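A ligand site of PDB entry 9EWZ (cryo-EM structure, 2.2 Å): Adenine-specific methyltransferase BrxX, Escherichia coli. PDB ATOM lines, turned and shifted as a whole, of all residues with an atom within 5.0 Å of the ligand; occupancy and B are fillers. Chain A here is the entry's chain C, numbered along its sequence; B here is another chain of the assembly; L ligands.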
ATOM      1  N   TYR A 218      17.727   3.240  -4.477  1.00  0.00           N
ATOM      2  CA  TYR A 218      17.333   2.061  -3.714  1.00  0.00           C
ATOM      3  C   TYR A 218      17.699   0.776  -4.440  1.00  0.00           C
ATOM      4  O   TYR A 218      17.969  -0.246  -3.799  1.00  0.00           O
ATOM      5  CB  TYR A 218      15.840   2.116  -3.429  1.00  0.00           C
ATOM      6  CG  TYR A 218      15.194   0.796  -3.066  1.00  0.00           C
ATOM      7  CD1 TYR A 218      15.310   0.278  -1.783  1.00  0.00           C
ATOM      8  CD2 TYR A 218      14.459   0.080  -3.995  1.00  0.00           C
ATOM      9  CE1 TYR A 218      14.713  -0.920  -1.444  1.00  0.00           C
ATOM     10  CE2 TYR A 218      13.867  -1.119  -3.677  1.00  0.00           C
ATOM     11  CZ  TYR A 218      13.998  -1.610  -2.397  1.00  0.00           C
ATOM     12  OH  TYR A 218      13.401  -2.805  -2.072  1.00  0.00           O
ATOM     13  N   ILE A 239      18.873 -11.620   2.794  1.00  0.00           N
ATOM     14  CA  ILE A 239      17.578 -11.730   2.114  1.00  0.00           C
ATOM     15  C   ILE A 239      17.193 -10.444   1.390  1.00  0.00           C
ATOM     16  O   ILE A 239      16.795 -10.515   0.218  1.00  0.00           O
ATOM     17  CB  ILE A 239      16.501 -12.215   3.097  1.00  0.00           C
ATOM     18  CG1 ILE A 239      16.704 -13.693   3.432  1.00  0.00           C
ATOM     19  CG2 ILE A 239      15.109 -11.974   2.533  1.00  0.00           C
ATOM     20  CD1 ILE A 239      15.672 -14.241   4.387  1.00  0.00           C
ATOM     21  N   PRO A 240      17.254  -9.265   2.016  1.00  0.00           N
ATOM     22  CA  PRO A 240      16.920  -8.045   1.256  1.00  0.00           C
ATOM     23  C   PRO A 240      17.825  -7.789   0.058  1.00  0.00           C
ATOM     24  O   PRO A 240      17.341  -7.297  -0.963  1.00  0.00           O
ATOM     25  CB  PRO A 240      17.052  -6.933   2.304  1.00  0.00           C
ATOM     26  CG  PRO A 240      17.916  -7.501   3.363  1.00  0.00           C
ATOM     27  CD  PRO A 240      17.570  -8.943   3.420  1.00  0.00           C
ATOM     28  N   THR A 243      16.508  -9.387  -3.173  1.00  0.00           N
ATOM     29  CA  THR A 243      15.112  -9.198  -3.566  1.00  0.00           C
ATOM     30  C   THR A 243      14.713  -7.715  -3.607  1.00  0.00           C
ATOM     31  O   THR A 243      13.531  -7.394  -3.425  1.00  0.00           O
ATOM     32  CB  THR A 243      14.159  -9.936  -2.620  1.00  0.00           C
ATOM     33  OG1 THR A 243      14.395  -9.519  -1.271  1.00  0.00           O
ATOM     34  CG2 THR A 243      14.350 -11.439  -2.725  1.00  0.00           C
ATOM     35  N   GLN A 244      15.665  -6.822  -3.854  1.00  0.00           N
ATOM     36  CA  GLN A 244      15.387  -5.386  -3.861  1.00  0.00           C
ATOM     37  C   GLN A 244      15.490  -4.862  -5.293  1.00  0.00           C
ATOM     38  O   GLN A 244      16.591  -4.714  -5.836  1.00  0.00           O
ATOM     39  CB  GLN A 244      16.347  -4.639  -2.942  1.00  0.00           C
ATOM     40  CG  GLN A 244      15.901  -4.644  -1.487  1.00  0.00           C
ATOM     41  CD  GLN A 244      16.911  -4.012  -0.554  1.00  0.00           C
ATOM     42  OE1 GLN A 244      18.068  -3.808  -0.922  1.00  0.00           O
ATOM     43  NE2 GLN A 244      16.480  -3.708   0.665  1.00  0.00           N
ATOM     44  N   LEU A 245      14.329  -4.590  -5.903  1.00  0.00           N
ATOM     45  CA  LEU A 245      14.233  -4.053  -7.247  1.00  0.00           C
ATOM     46  C   LEU A 245      13.252  -2.882  -7.243  1.00  0.00           C
ATOM     47  O   LEU A 245      12.541  -2.638  -6.270  1.00  0.00           O
ATOM     48  CB  LEU A 245      13.774  -5.124  -8.250  1.00  0.00           C
ATOM     49  CG  LEU A 245      14.758  -6.228  -8.673  1.00  0.00           C
ATOM     50  CD1 LEU A 245      16.113  -5.647  -9.041  1.00  0.00           C
ATOM     51  CD2 LEU A 245      14.892  -7.306  -7.608  1.00  0.00           C
ATOM     52  N   PHE A 246      13.232  -2.153  -8.358  1.00  0.00           N
ATOM     53  CA  PHE A 246      12.358  -0.995  -8.524  1.00  0.00           C
ATOM     54  C   PHE A 246      11.297  -1.307  -9.573  1.00  0.00           C
ATOM     55  O   PHE A 246      11.630  -1.700 -10.700  1.00  0.00           O
ATOM     56  CB  PHE A 246      13.170   0.239  -8.936  1.00  0.00           C
ATOM     57  CG  PHE A 246      12.398   1.524  -8.874  1.00  0.00           C
ATOM     58  CD1 PHE A 246      11.707   1.882  -7.728  1.00  0.00           C
ATOM     59  CD2 PHE A 246      12.386   2.389  -9.956  1.00  0.00           C
ATOM     60  CE1 PHE A 246      11.001   3.070  -7.676  1.00  0.00           C
ATOM     61  CE2 PHE A 246      11.686   3.584  -9.904  1.00  0.00           C
ATOM     62  CZ  PHE A 246      10.993   3.919  -8.761  1.00  0.00           C
ATOM     63  N   THR A 247      10.029  -1.157  -9.196  1.00  0.00           N
ATOM     64  CA  THR A 247       8.912  -1.530 -10.055  1.00  0.00           C
ATOM     65  C   THR A 247       8.610  -0.433 -11.066  1.00  0.00           C
ATOM     66  O   THR A 247       8.606   0.753 -10.706  1.00  0.00           O
ATOM     67  CB  THR A 247       7.662  -1.812  -9.208  1.00  0.00           C
ATOM     68  OG1 THR A 247       8.027  -2.634  -8.086  1.00  0.00           O
ATOM     69  CG2 THR A 247       6.610  -2.533 -10.034  1.00  0.00           C
ATOM     70  N   ASP A 311       1.063  -1.787   2.267  1.00  0.00           N
ATOM     71  CA  ASP A 311       2.112  -2.370   1.446  1.00  0.00           C
ATOM     72  C   ASP A 311       2.965  -3.288   2.321  1.00  0.00           C
ATOM     73  O   ASP A 311       3.800  -2.798   3.101  1.00  0.00           O
ATOM     74  CB  ASP A 311       2.977  -1.280   0.809  1.00  0.00           C
ATOM     75  CG  ASP A 311       3.768  -1.787  -0.390  1.00  0.00           C
ATOM     76  OD1 ASP A 311       4.007  -3.011  -0.476  1.00  0.00           O
ATOM     77  OD2 ASP A 311       4.149  -0.959  -1.243  1.00  0.00           O
ATOM     78  N   PRO A 312       2.780  -4.608   2.236  1.00  0.00           N
ATOM     79  CA  PRO A 312       3.541  -5.513   3.117  1.00  0.00           C
ATOM     80  C   PRO A 312       5.035  -5.493   2.863  1.00  0.00           C
ATOM     81  O   PRO A 312       5.806  -5.882   3.751  1.00  0.00           O
ATOM     82  CB  PRO A 312       2.948  -6.890   2.810  1.00  0.00           C
ATOM     83  CG  PRO A 312       1.643  -6.614   2.132  1.00  0.00           C
ATOM     84  CD  PRO A 312       1.833  -5.336   1.384  1.00  0.00           C
ATOM     85  N   ALA A 313       5.475  -5.080   1.670  1.00  0.00           N
ATOM     86  CA  ALA A 313       6.900  -4.908   1.356  1.00  0.00           C
ATOM     87  C   ALA A 313       7.026  -3.567   0.650  1.00  0.00           C
ATOM     88  O   ALA A 313       6.992  -3.508  -0.585  1.00  0.00           O
ATOM     89  CB  ALA A 313       7.422  -6.058   0.519  1.00  0.00           C
ATOM     90  N   CYS A 314       7.170  -2.500   1.421  1.00  0.00           N
ATOM     91  CA  CYS A 314       7.085  -1.158   0.864  1.00  0.00           C
ATOM     92  C   CYS A 314       8.275  -0.842  -0.031  1.00  0.00           C
ATOM     93  O   CYS A 314       8.113  -0.226  -1.088  1.00  0.00           O
ATOM     94  CB  CYS A 314       6.957  -0.123   1.985  1.00  0.00           C
ATOM     95  SG  CYS A 314       8.352  -0.072   3.132  1.00  0.00           S
ATOM     96  N   GLY A 315       9.477  -1.251   0.369  1.00  0.00           N
ATOM     97  CA  GLY A 315      10.664  -0.951  -0.414  1.00  0.00           C
ATOM     98  C   GLY A 315      10.968   0.531  -0.482  1.00  0.00           C
ATOM     99  O   GLY A 315      11.256   1.156   0.548  1.00  0.00           O
ATOM    100  N   SER A 316      10.897   1.103  -1.678  1.00  0.00           N
ATOM    101  CA  SER A 316      11.150   2.527  -1.862  1.00  0.00           C
ATOM    102  C   SER A 316       9.876   3.375  -1.754  1.00  0.00           C
ATOM    103  O   SER A 316       9.983   4.604  -1.762  1.00  0.00           O
ATOM    104  CB  SER A 316      11.814   2.780  -3.211  1.00  0.00           C
ATOM    105  OG  SER A 316      11.024   2.284  -4.276  1.00  0.00           O
ATOM    106  N   GLY A 317       8.708   2.753  -1.657  1.00  0.00           N
ATOM    107  CA  GLY A 317       7.474   3.500  -1.483  1.00  0.00           C
ATOM    108  C   GLY A 317       6.774   3.942  -2.746  1.00  0.00           C
ATOM    109  O   GLY A 317       5.944   4.859  -2.679  1.00  0.00           O
ATOM    110  N   HIS A 318       7.071   3.326  -3.883  1.00  0.00           N
ATOM    111  CA  HIS A 318       6.439   3.707  -5.145  1.00  0.00           C
ATOM    112  C   HIS A 318       4.925   3.470  -5.107  1.00  0.00           C
ATOM    113  O   HIS A 318       4.129   4.350  -5.479  1.00  0.00           O
ATOM    114  CB  HIS A 318       7.083   2.917  -6.287  1.00  0.00           C
ATOM    115  CG  HIS A 318       6.936   3.568  -7.632  1.00  0.00           C
ATOM    116  ND1 HIS A 318       7.392   2.974  -8.782  1.00  0.00           N
ATOM    117  CD2 HIS A 318       6.393   4.748  -8.005  1.00  0.00           C
ATOM    118  CE1 HIS A 318       7.126   3.760  -9.813  1.00  0.00           C
ATOM    119  NE2 HIS A 318       6.522   4.844  -9.365  1.00  0.00           N
ATOM    120  N   ILE A 319       4.525   2.293  -4.645  1.00  0.00           N
ATOM    121  CA  ILE A 319       3.109   1.948  -4.561  1.00  0.00           C
ATOM    122  C   ILE A 319       2.389   2.907  -3.627  1.00  0.00           C
ATOM    123  O   ILE A 319       1.256   3.329  -3.901  1.00  0.00           O
ATOM    124  CB  ILE A 319       2.939   0.488  -4.122  1.00  0.00           C
ATOM    125  CG1 ILE A 319       3.557  -0.459  -5.151  1.00  0.00           C
ATOM    126  CG2 ILE A 319       1.481   0.156  -3.888  1.00  0.00           C
ATOM    127  CD1 ILE A 319       3.455  -1.910  -4.801  1.00  0.00           C
ATOM    128  N   ASP A 354       8.284  -3.243   6.106  1.00  0.00           N
ATOM    129  CA  ASP A 354       9.419  -3.814   5.396  1.00  0.00           C
ATOM    130  C   ASP A 354      10.332  -4.534   6.378  1.00  0.00           C
ATOM    131  O   ASP A 354      10.263  -4.322   7.590  1.00  0.00           O
ATOM    132  CB  ASP A 354      10.202  -2.749   4.617  1.00  0.00           C
ATOM    133  CG  ASP A 354      10.979  -3.331   3.458  1.00  0.00           C
ATOM    134  OD1 ASP A 354      11.778  -4.267   3.672  1.00  0.00           O
ATOM    135  OD2 ASP A 354      10.785  -2.861   2.315  1.00  0.00           O
ATOM    136  N   ILE A 355      11.188  -5.396   5.834  1.00  0.00           N
ATOM    137  CA  ILE A 355      12.128  -6.166   6.646  1.00  0.00           C
ATOM    138  C   ILE A 355      13.506  -5.515   6.717  1.00  0.00           C
ATOM    139  O   ILE A 355      14.351  -5.991   7.488  1.00  0.00           O
ATOM    140  CB  ILE A 355      12.239  -7.622   6.124  1.00  0.00           C
ATOM    141  CG1 ILE A 355      12.600  -8.577   7.257  1.00  0.00           C
ATOM    142  CG2 ILE A 355      13.249  -7.714   4.990  1.00  0.00           C
ATOM    143  CD1 ILE A 355      12.628 -10.030   6.832  1.00  0.00           C
ATOM    144  N   ASP A 356      13.742  -4.453   5.962  1.00  0.00           N
ATOM    145  CA  ASP A 356      15.031  -3.775   5.926  1.00  0.00           C
ATOM    146  C   ASP A 356      14.868  -2.329   6.388  1.00  0.00           C
ATOM    147  O   ASP A 356      13.898  -1.657   6.004  1.00  0.00           O
ATOM    148  CB  ASP A 356      15.634  -3.822   4.520  1.00  0.00           C
ATOM    149  CG  ASP A 356      17.094  -3.433   4.500  1.00  0.00           C
ATOM    150  OD1 ASP A 356      17.718  -3.386   5.585  1.00  0.00           O
ATOM    151  OD2 ASP A 356      17.626  -3.171   3.397  1.00  0.00           O
ATOM    152  N   ALA A 359      15.120   0.400   3.475  1.00  0.00           N
ATOM    153  CA  ALA A 359      13.870   0.583   2.736  1.00  0.00           C
ATOM    154  C   ALA A 359      12.893   1.446   3.513  1.00  0.00           C
ATOM    155  O   ALA A 359      12.207   2.291   2.919  1.00  0.00           O
ATOM    156  CB  ALA A 359      13.249  -0.781   2.416  1.00  0.00           C
ATOM    157  N   LEU A 390      10.324  -4.173  10.432  1.00  0.00           N
ATOM    158  CA  LEU A 390      10.051  -5.154  11.468  1.00  0.00           C
ATOM    159  C   LEU A 390      11.293  -5.390  12.321  1.00  0.00           C
ATOM    160  O   LEU A 390      12.398  -5.573  11.798  1.00  0.00           O
ATOM    161  CB  LEU A 390       9.581  -6.467  10.846  1.00  0.00           C
ATOM    162  CG  LEU A 390       8.247  -6.369  10.100  1.00  0.00           C
ATOM    163  CD1 LEU A 390       8.389  -6.854   8.676  1.00  0.00           C
ATOM    164  CD2 LEU A 390       7.172  -7.140  10.838  1.00  0.00           C
ATOM    165  N   THR A 448      13.619 -12.849   9.882  1.00  0.00           N
ATOM    166  CA  THR A 448      13.588 -13.929   8.907  1.00  0.00           C
ATOM    167  C   THR A 448      12.222 -14.102   8.259  1.00  0.00           C
ATOM    168  O   THR A 448      12.149 -14.391   7.060  1.00  0.00           O
ATOM    169  CB  THR A 448      13.993 -15.250   9.570  1.00  0.00           C
ATOM    170  OG1 THR A 448      15.260 -15.084  10.228  1.00  0.00           O
ATOM    171  CG2 THR A 448      14.129 -16.359   8.531  1.00  0.00           C
ATOM    172  N   LEU A 449      11.142 -13.912   9.012  1.00  0.00           N
ATOM    173  CA  LEU A 449       9.799 -14.113   8.489  1.00  0.00           C
ATOM    174  C   LEU A 449       9.185 -12.827   7.943  1.00  0.00           C
ATOM    175  O   LEU A 449       8.539 -12.860   6.889  1.00  0.00           O
ATOM    176  CB  LEU A 449       8.894 -14.703   9.585  1.00  0.00           C
ATOM    177  CG  LEU A 449       9.446 -15.956  10.270  1.00  0.00           C
ATOM    178  CD1 LEU A 449       8.476 -16.466  11.317  1.00  0.00           C
ATOM    179  CD2 LEU A 449       9.766 -17.029   9.242  1.00  0.00           C
ATOM    180  N   GLY A 450       9.370 -11.716   8.628  1.00  0.00           N
ATOM    181  CA  GLY A 450       8.880 -10.450   8.105  1.00  0.00           C
ATOM    182  C   GLY A 450       7.377 -10.302   8.295  1.00  0.00           C
ATOM    183  O   GLY A 450       6.862 -10.459   9.399  1.00  0.00           O
ATOM    184  N   SER A 451       6.686 -10.006   7.206  1.00  0.00           N
ATOM    185  CA  SER A 451       5.252  -9.732   7.237  1.00  0.00           C
ATOM    186  C   SER A 451       4.404 -10.998   7.222  1.00  0.00           C
ATOM    187  O   SER A 451       3.172 -10.891   7.259  1.00  0.00           O
ATOM    188  CB  SER A 451       4.862  -8.838   6.060  1.00  0.00           C
ATOM    189  OG  SER A 451       5.555  -7.601   6.108  1.00  0.00           O
ATOM    190  N   ASN A 508       4.663  -5.846  -4.415  1.00  0.00           N
ATOM    191  CA  ASN A 508       5.540  -6.539  -5.351  1.00  0.00           C
ATOM    192  C   ASN A 508       6.405  -7.452  -4.495  1.00  0.00           C
ATOM    193  O   ASN A 508       7.481  -7.044  -4.032  1.00  0.00           O
ATOM    194  CB  ASN A 508       6.371  -5.566  -6.169  1.00  0.00           C
ATOM    195  CG  ASN A 508       7.329  -6.261  -7.123  1.00  0.00           C
ATOM    196  OD1 ASN A 508       7.150  -7.422  -7.458  1.00  0.00           O
ATOM    197  ND2 ASN A 508       8.352  -5.548  -7.563  1.00  0.00           N
ATOM    198  N   PRO A 509       5.979  -8.690  -4.264  1.00  0.00           N
ATOM    199  CA  PRO A 509       6.630  -9.519  -3.247  1.00  0.00           C
ATOM    200  C   PRO A 509       8.007  -9.959  -3.682  1.00  0.00           C
ATOM    201  O   PRO A 509       8.341  -9.925  -4.872  1.00  0.00           O
ATOM    202  CB  PRO A 509       5.680 -10.732  -3.122  1.00  0.00           C
ATOM    203  CG  PRO A 509       4.425 -10.333  -3.825  1.00  0.00           C
ATOM    204  CD  PRO A 509       4.847  -9.373  -4.887  1.00  0.00           C
ATOM    205  N   PRO A 510       8.869 -10.358  -2.735  1.00  0.00           N
ATOM    206  CA  PRO A 510      10.144 -10.975  -3.104  1.00  0.00           C
ATOM    207  C   PRO A 510       9.944 -12.320  -3.764  1.00  0.00           C
ATOM    208  O   PRO A 510       9.008 -13.062  -3.461  1.00  0.00           O
ATOM    209  CB  PRO A 510      10.865 -11.110  -1.763  1.00  0.00           C
ATOM    210  CG  PRO A 510       9.772 -11.153  -0.756  1.00  0.00           C
ATOM    211  CD  PRO A 510       8.702 -10.249  -1.277  1.00  0.00           C
ATOM    212  N   LEU A 536       8.414 -17.954  -2.102  1.00  0.00           N
ATOM    213  CA  LEU A 536       8.091 -16.840  -1.220  1.00  0.00           C
ATOM    214  C   LEU A 536       6.925 -16.011  -1.747  1.00  0.00           C
ATOM    215  O   LEU A 536       6.071 -15.567  -0.966  1.00  0.00           O
ATOM    216  CB  LEU A 536       9.333 -15.969  -1.024  1.00  0.00           C
ATOM    217  CG  LEU A 536       9.517 -15.232   0.303  1.00  0.00           C
ATOM    218  CD1 LEU A 536       9.418 -16.199   1.461  1.00  0.00           C
ATOM    219  CD2 LEU A 536      10.839 -14.511   0.324  1.00  0.00           C
ATOM    220  N   PHE A 540       3.366 -14.992   0.092  1.00  0.00           N
ATOM    221  CA  PHE A 540       2.828 -13.640   0.200  1.00  0.00           C
ATOM    222  C   PHE A 540       1.437 -13.555  -0.407  1.00  0.00           C
ATOM    223  O   PHE A 540       0.539 -12.914   0.149  1.00  0.00           O
ATOM    224  CB  PHE A 540       3.764 -12.637  -0.461  1.00  0.00           C
ATOM    225  CG  PHE A 540       4.719 -11.985   0.488  1.00  0.00           C
ATOM    226  CD1 PHE A 540       5.905 -12.601   0.844  1.00  0.00           C
ATOM    227  CD2 PHE A 540       4.434 -10.738   1.011  1.00  0.00           C
ATOM    228  CE1 PHE A 540       6.779 -12.001   1.719  1.00  0.00           C
ATOM    229  CE2 PHE A 540       5.315 -10.130   1.888  1.00  0.00           C
ATOM    230  CZ  PHE A 540       6.488 -10.761   2.241  1.00  0.00           C
ATOM    231  P    DA B  10      15.153 -17.894  -8.163  1.00  0.00           P
ATOM    232  OP1  DA B  10      16.366 -17.762  -7.340  1.00  0.00           O
ATOM    233  OP2  DA B  10      13.835 -18.030  -7.505  1.00  0.00           O
ATOM    234  O5'  DA B  10      15.095 -16.639  -9.152  1.00  0.00           O
ATOM    235  C5'  DA B  10      14.816 -15.340  -8.650  1.00  0.00           C
ATOM    236  C4'  DA B  10      14.992 -14.303  -9.745  1.00  0.00           C
ATOM    237  O4'  DA B  10      13.993 -13.265  -9.581  1.00  0.00           O
ATOM    238  C3'  DA B  10      16.337 -13.585  -9.745  1.00  0.00           C
ATOM    239  O3'  DA B  10      16.644 -13.192 -11.081  1.00  0.00           O
ATOM    240  C2'  DA B  10      16.047 -12.380  -8.857  1.00  0.00           C
ATOM    241  C1'  DA B  10      14.635 -12.034  -9.300  1.00  0.00           C
ATOM    242  N9   DA B  10      13.838 -11.343  -8.291  1.00  0.00           N
ATOM    243  C8   DA B  10      13.790 -11.603  -6.950  1.00  0.00           C
ATOM    244  N7   DA B  10      12.968 -10.830  -6.295  1.00  0.00           N
ATOM    245  C5   DA B  10      12.433 -10.004  -7.265  1.00  0.00           C
ATOM    246  C6   DA B  10      11.490  -8.956  -7.212  1.00  0.00           C
ATOM    247  N6   DA B  10      10.908  -8.557  -6.085  1.00  0.00           N
ATOM    248  N1   DA B  10      11.179  -8.339  -8.367  1.00  0.00           N
ATOM    249  C2   DA B  10      11.771  -8.747  -9.494  1.00  0.00           C
ATOM    250  N3   DA B  10      12.661  -9.715  -9.667  1.00  0.00           N
ATOM    251  C4   DA B  10      12.963 -10.311  -8.502  1.00  0.00           C
HETATM  252  N1  LIG L   1       7.354  -2.408  -4.687  1.00  0.00           N
HETATM  253  C1  LIG L   1       8.426  -1.644  -4.068  1.00  0.00           C
HETATM  254  C2  LIG L   1       9.223  -0.861  -5.099  1.00  0.00           C
HETATM  255  O1  LIG L   1       9.100  -1.078  -6.304  1.00  0.00           O
HETATM  256  O2  LIG L   1      10.017   0.022  -4.760  1.00  0.00           O
HETATM  257  C3  LIG L   1       9.343  -2.566  -3.277  1.00  0.00           C
HETATM  258  C4  LIG L   1       9.464  -3.989  -3.808  1.00  0.00           C
HETATM  259  S1  LIG L   1      11.072  -4.725  -3.454  1.00  0.00           S
HETATM  260  C5  LIG L   1      11.356  -5.583  -5.017  1.00  0.00           C
HETATM  261  C6  LIG L   1      10.643  -6.114  -2.372  1.00  0.00           C
HETATM  262  C7  LIG L   1      10.968  -5.810  -0.913  1.00  0.00           C
HETATM  263  O3  LIG L   1      10.425  -6.791  -0.050  1.00  0.00           O
HETATM  264  C8  LIG L   1      12.464  -5.786  -0.630  1.00  0.00           C
HETATM  265  O4  LIG L   1      12.874  -4.460  -0.408  1.00  0.00           O
HETATM  266  C9  LIG L   1      12.648  -6.592   0.645  1.00  0.00           C
HETATM  267  O5  LIG L   1      13.340  -5.843   1.605  1.00  0.00           O
HETATM  268  C10 LIG L   1      11.232  -6.865   1.109  1.00  0.00           C
HETATM  269  N2  LIG L   1      11.098  -8.178   1.769  1.00  0.00           N
HETATM  270  C11 LIG L   1      11.790  -9.326   1.473  1.00  0.00           C
HETATM  271  N3  LIG L   1      11.365 -10.301   2.312  1.00  0.00           N
HETATM  272  C12 LIG L   1      10.418  -9.794   3.127  1.00  0.00           C
HETATM  273  C13 LIG L   1       9.663 -10.356   4.146  1.00  0.00           C
HETATM  274  N4  LIG L   1       9.823 -11.634   4.471  1.00  0.00           N
HETATM  275  N5  LIG L   1       8.742  -9.580   4.820  1.00  0.00           N
HETATM  276  C14 LIG L   1       8.581  -8.258   4.472  1.00  0.00           C
HETATM  277  N6  LIG L   1       9.334  -7.709   3.458  1.00  0.00           N
HETATM  278  C15 LIG L   1      10.240  -8.460   2.787  1.00  0.00           C
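OH of Tyr 218 lies within hydrogen-bond range of O4 of the ligand. O2 of the ligand is in hydrogen-bond range of N of Ser 316, 3.4 Å away. The side-chain hydroxyl (OG) of Ser 316 is in hydrogen-bond range of an oxygen (O2) of the ligand, at 2.5 Å. The backbone NH of Thr 247 is in hydrogen-bond range of an oxygen (O1) of the ligand (3.0 Å). The side-chain hydroxyl (OG1) of Thr 247 lies within hydrogen-bond range of an oxygen (O1) of the ligand (2.6 Å). O of Leu 449 lies within hydrogen-bond range of N4 of the ligand, at 3.0 Å. OD1 of Asp 354 lies within hydrogen-bond range of O5 of the ligand, 3.0 Å away. N of Ser 451 sits at hydrogen-bond distance from N5 of the ligand, at 3.2 Å.
ND2 of Asn 508 sits at hydrogen-bond distance from OG1 of Thr 247, 3.0 Å away. The side-chain sulfur of Cys 314 lies close to the side-chain carboxylate of Asp 354 (3.8 Å). The backbone NH of Gly 315 sits at hydrogen-bond distance from the side-chain carboxylate of Asp 354 (2.8 Å). The side-chain carboxylate of Asp 354 is in hydrogen-bond range of the backbone NH of Asp 356 (3.0 Å). O of Asp 354 lies within hydrogen-bond range of N of Leu 390 (2.8 Å). The backbone NH (N) of Ala 313 sits close to the side-chain carboxylate (OD1) of Asp 311. OG of Ser 451 is in hydrogen-bond range of O of Pro 312 (2.9 Å). OG1 of Thr 243 is in hydrogen-bond range of O of Ile 239 (3.0 Å).
A sulfur (S1) of the ligand lies close to the backbone carbonyl oxygen (O) of Thr 243, 3.6 Å away. Residues that only touch the ligand: Pro 240 (3.9 Å), Gln 244 (3.2 Å), Leu 245 (3.3 Å), Phe 246 (3.9 Å), Pro 312 (3.7 Å), Ala 313 (3.1 Å), Cys 314 (3.3 Å), Gly 315 (3.5 Å), Ile 319 (3.9 Å), Ile 355 (3.8 Å), Gly 450 (3.4 Å), Asn 508 (3.6 Å), Pro 510 (3.5 Å), Phe 540 (3.6 Å) and DA 10 of chain B (3.2 Å). Hydrophobic or aromatic side chains that line the ligand: Tyr 218, Pro 240, Phe 246, Ala 313, Ile 319, Ile 355, Pro 510 and Phe 540. Of the 32 residues printed, 22 come within 4 Å of the ligand. The nearest printed residue that does not touch the ligand is Ile 239 (4.1 Å).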
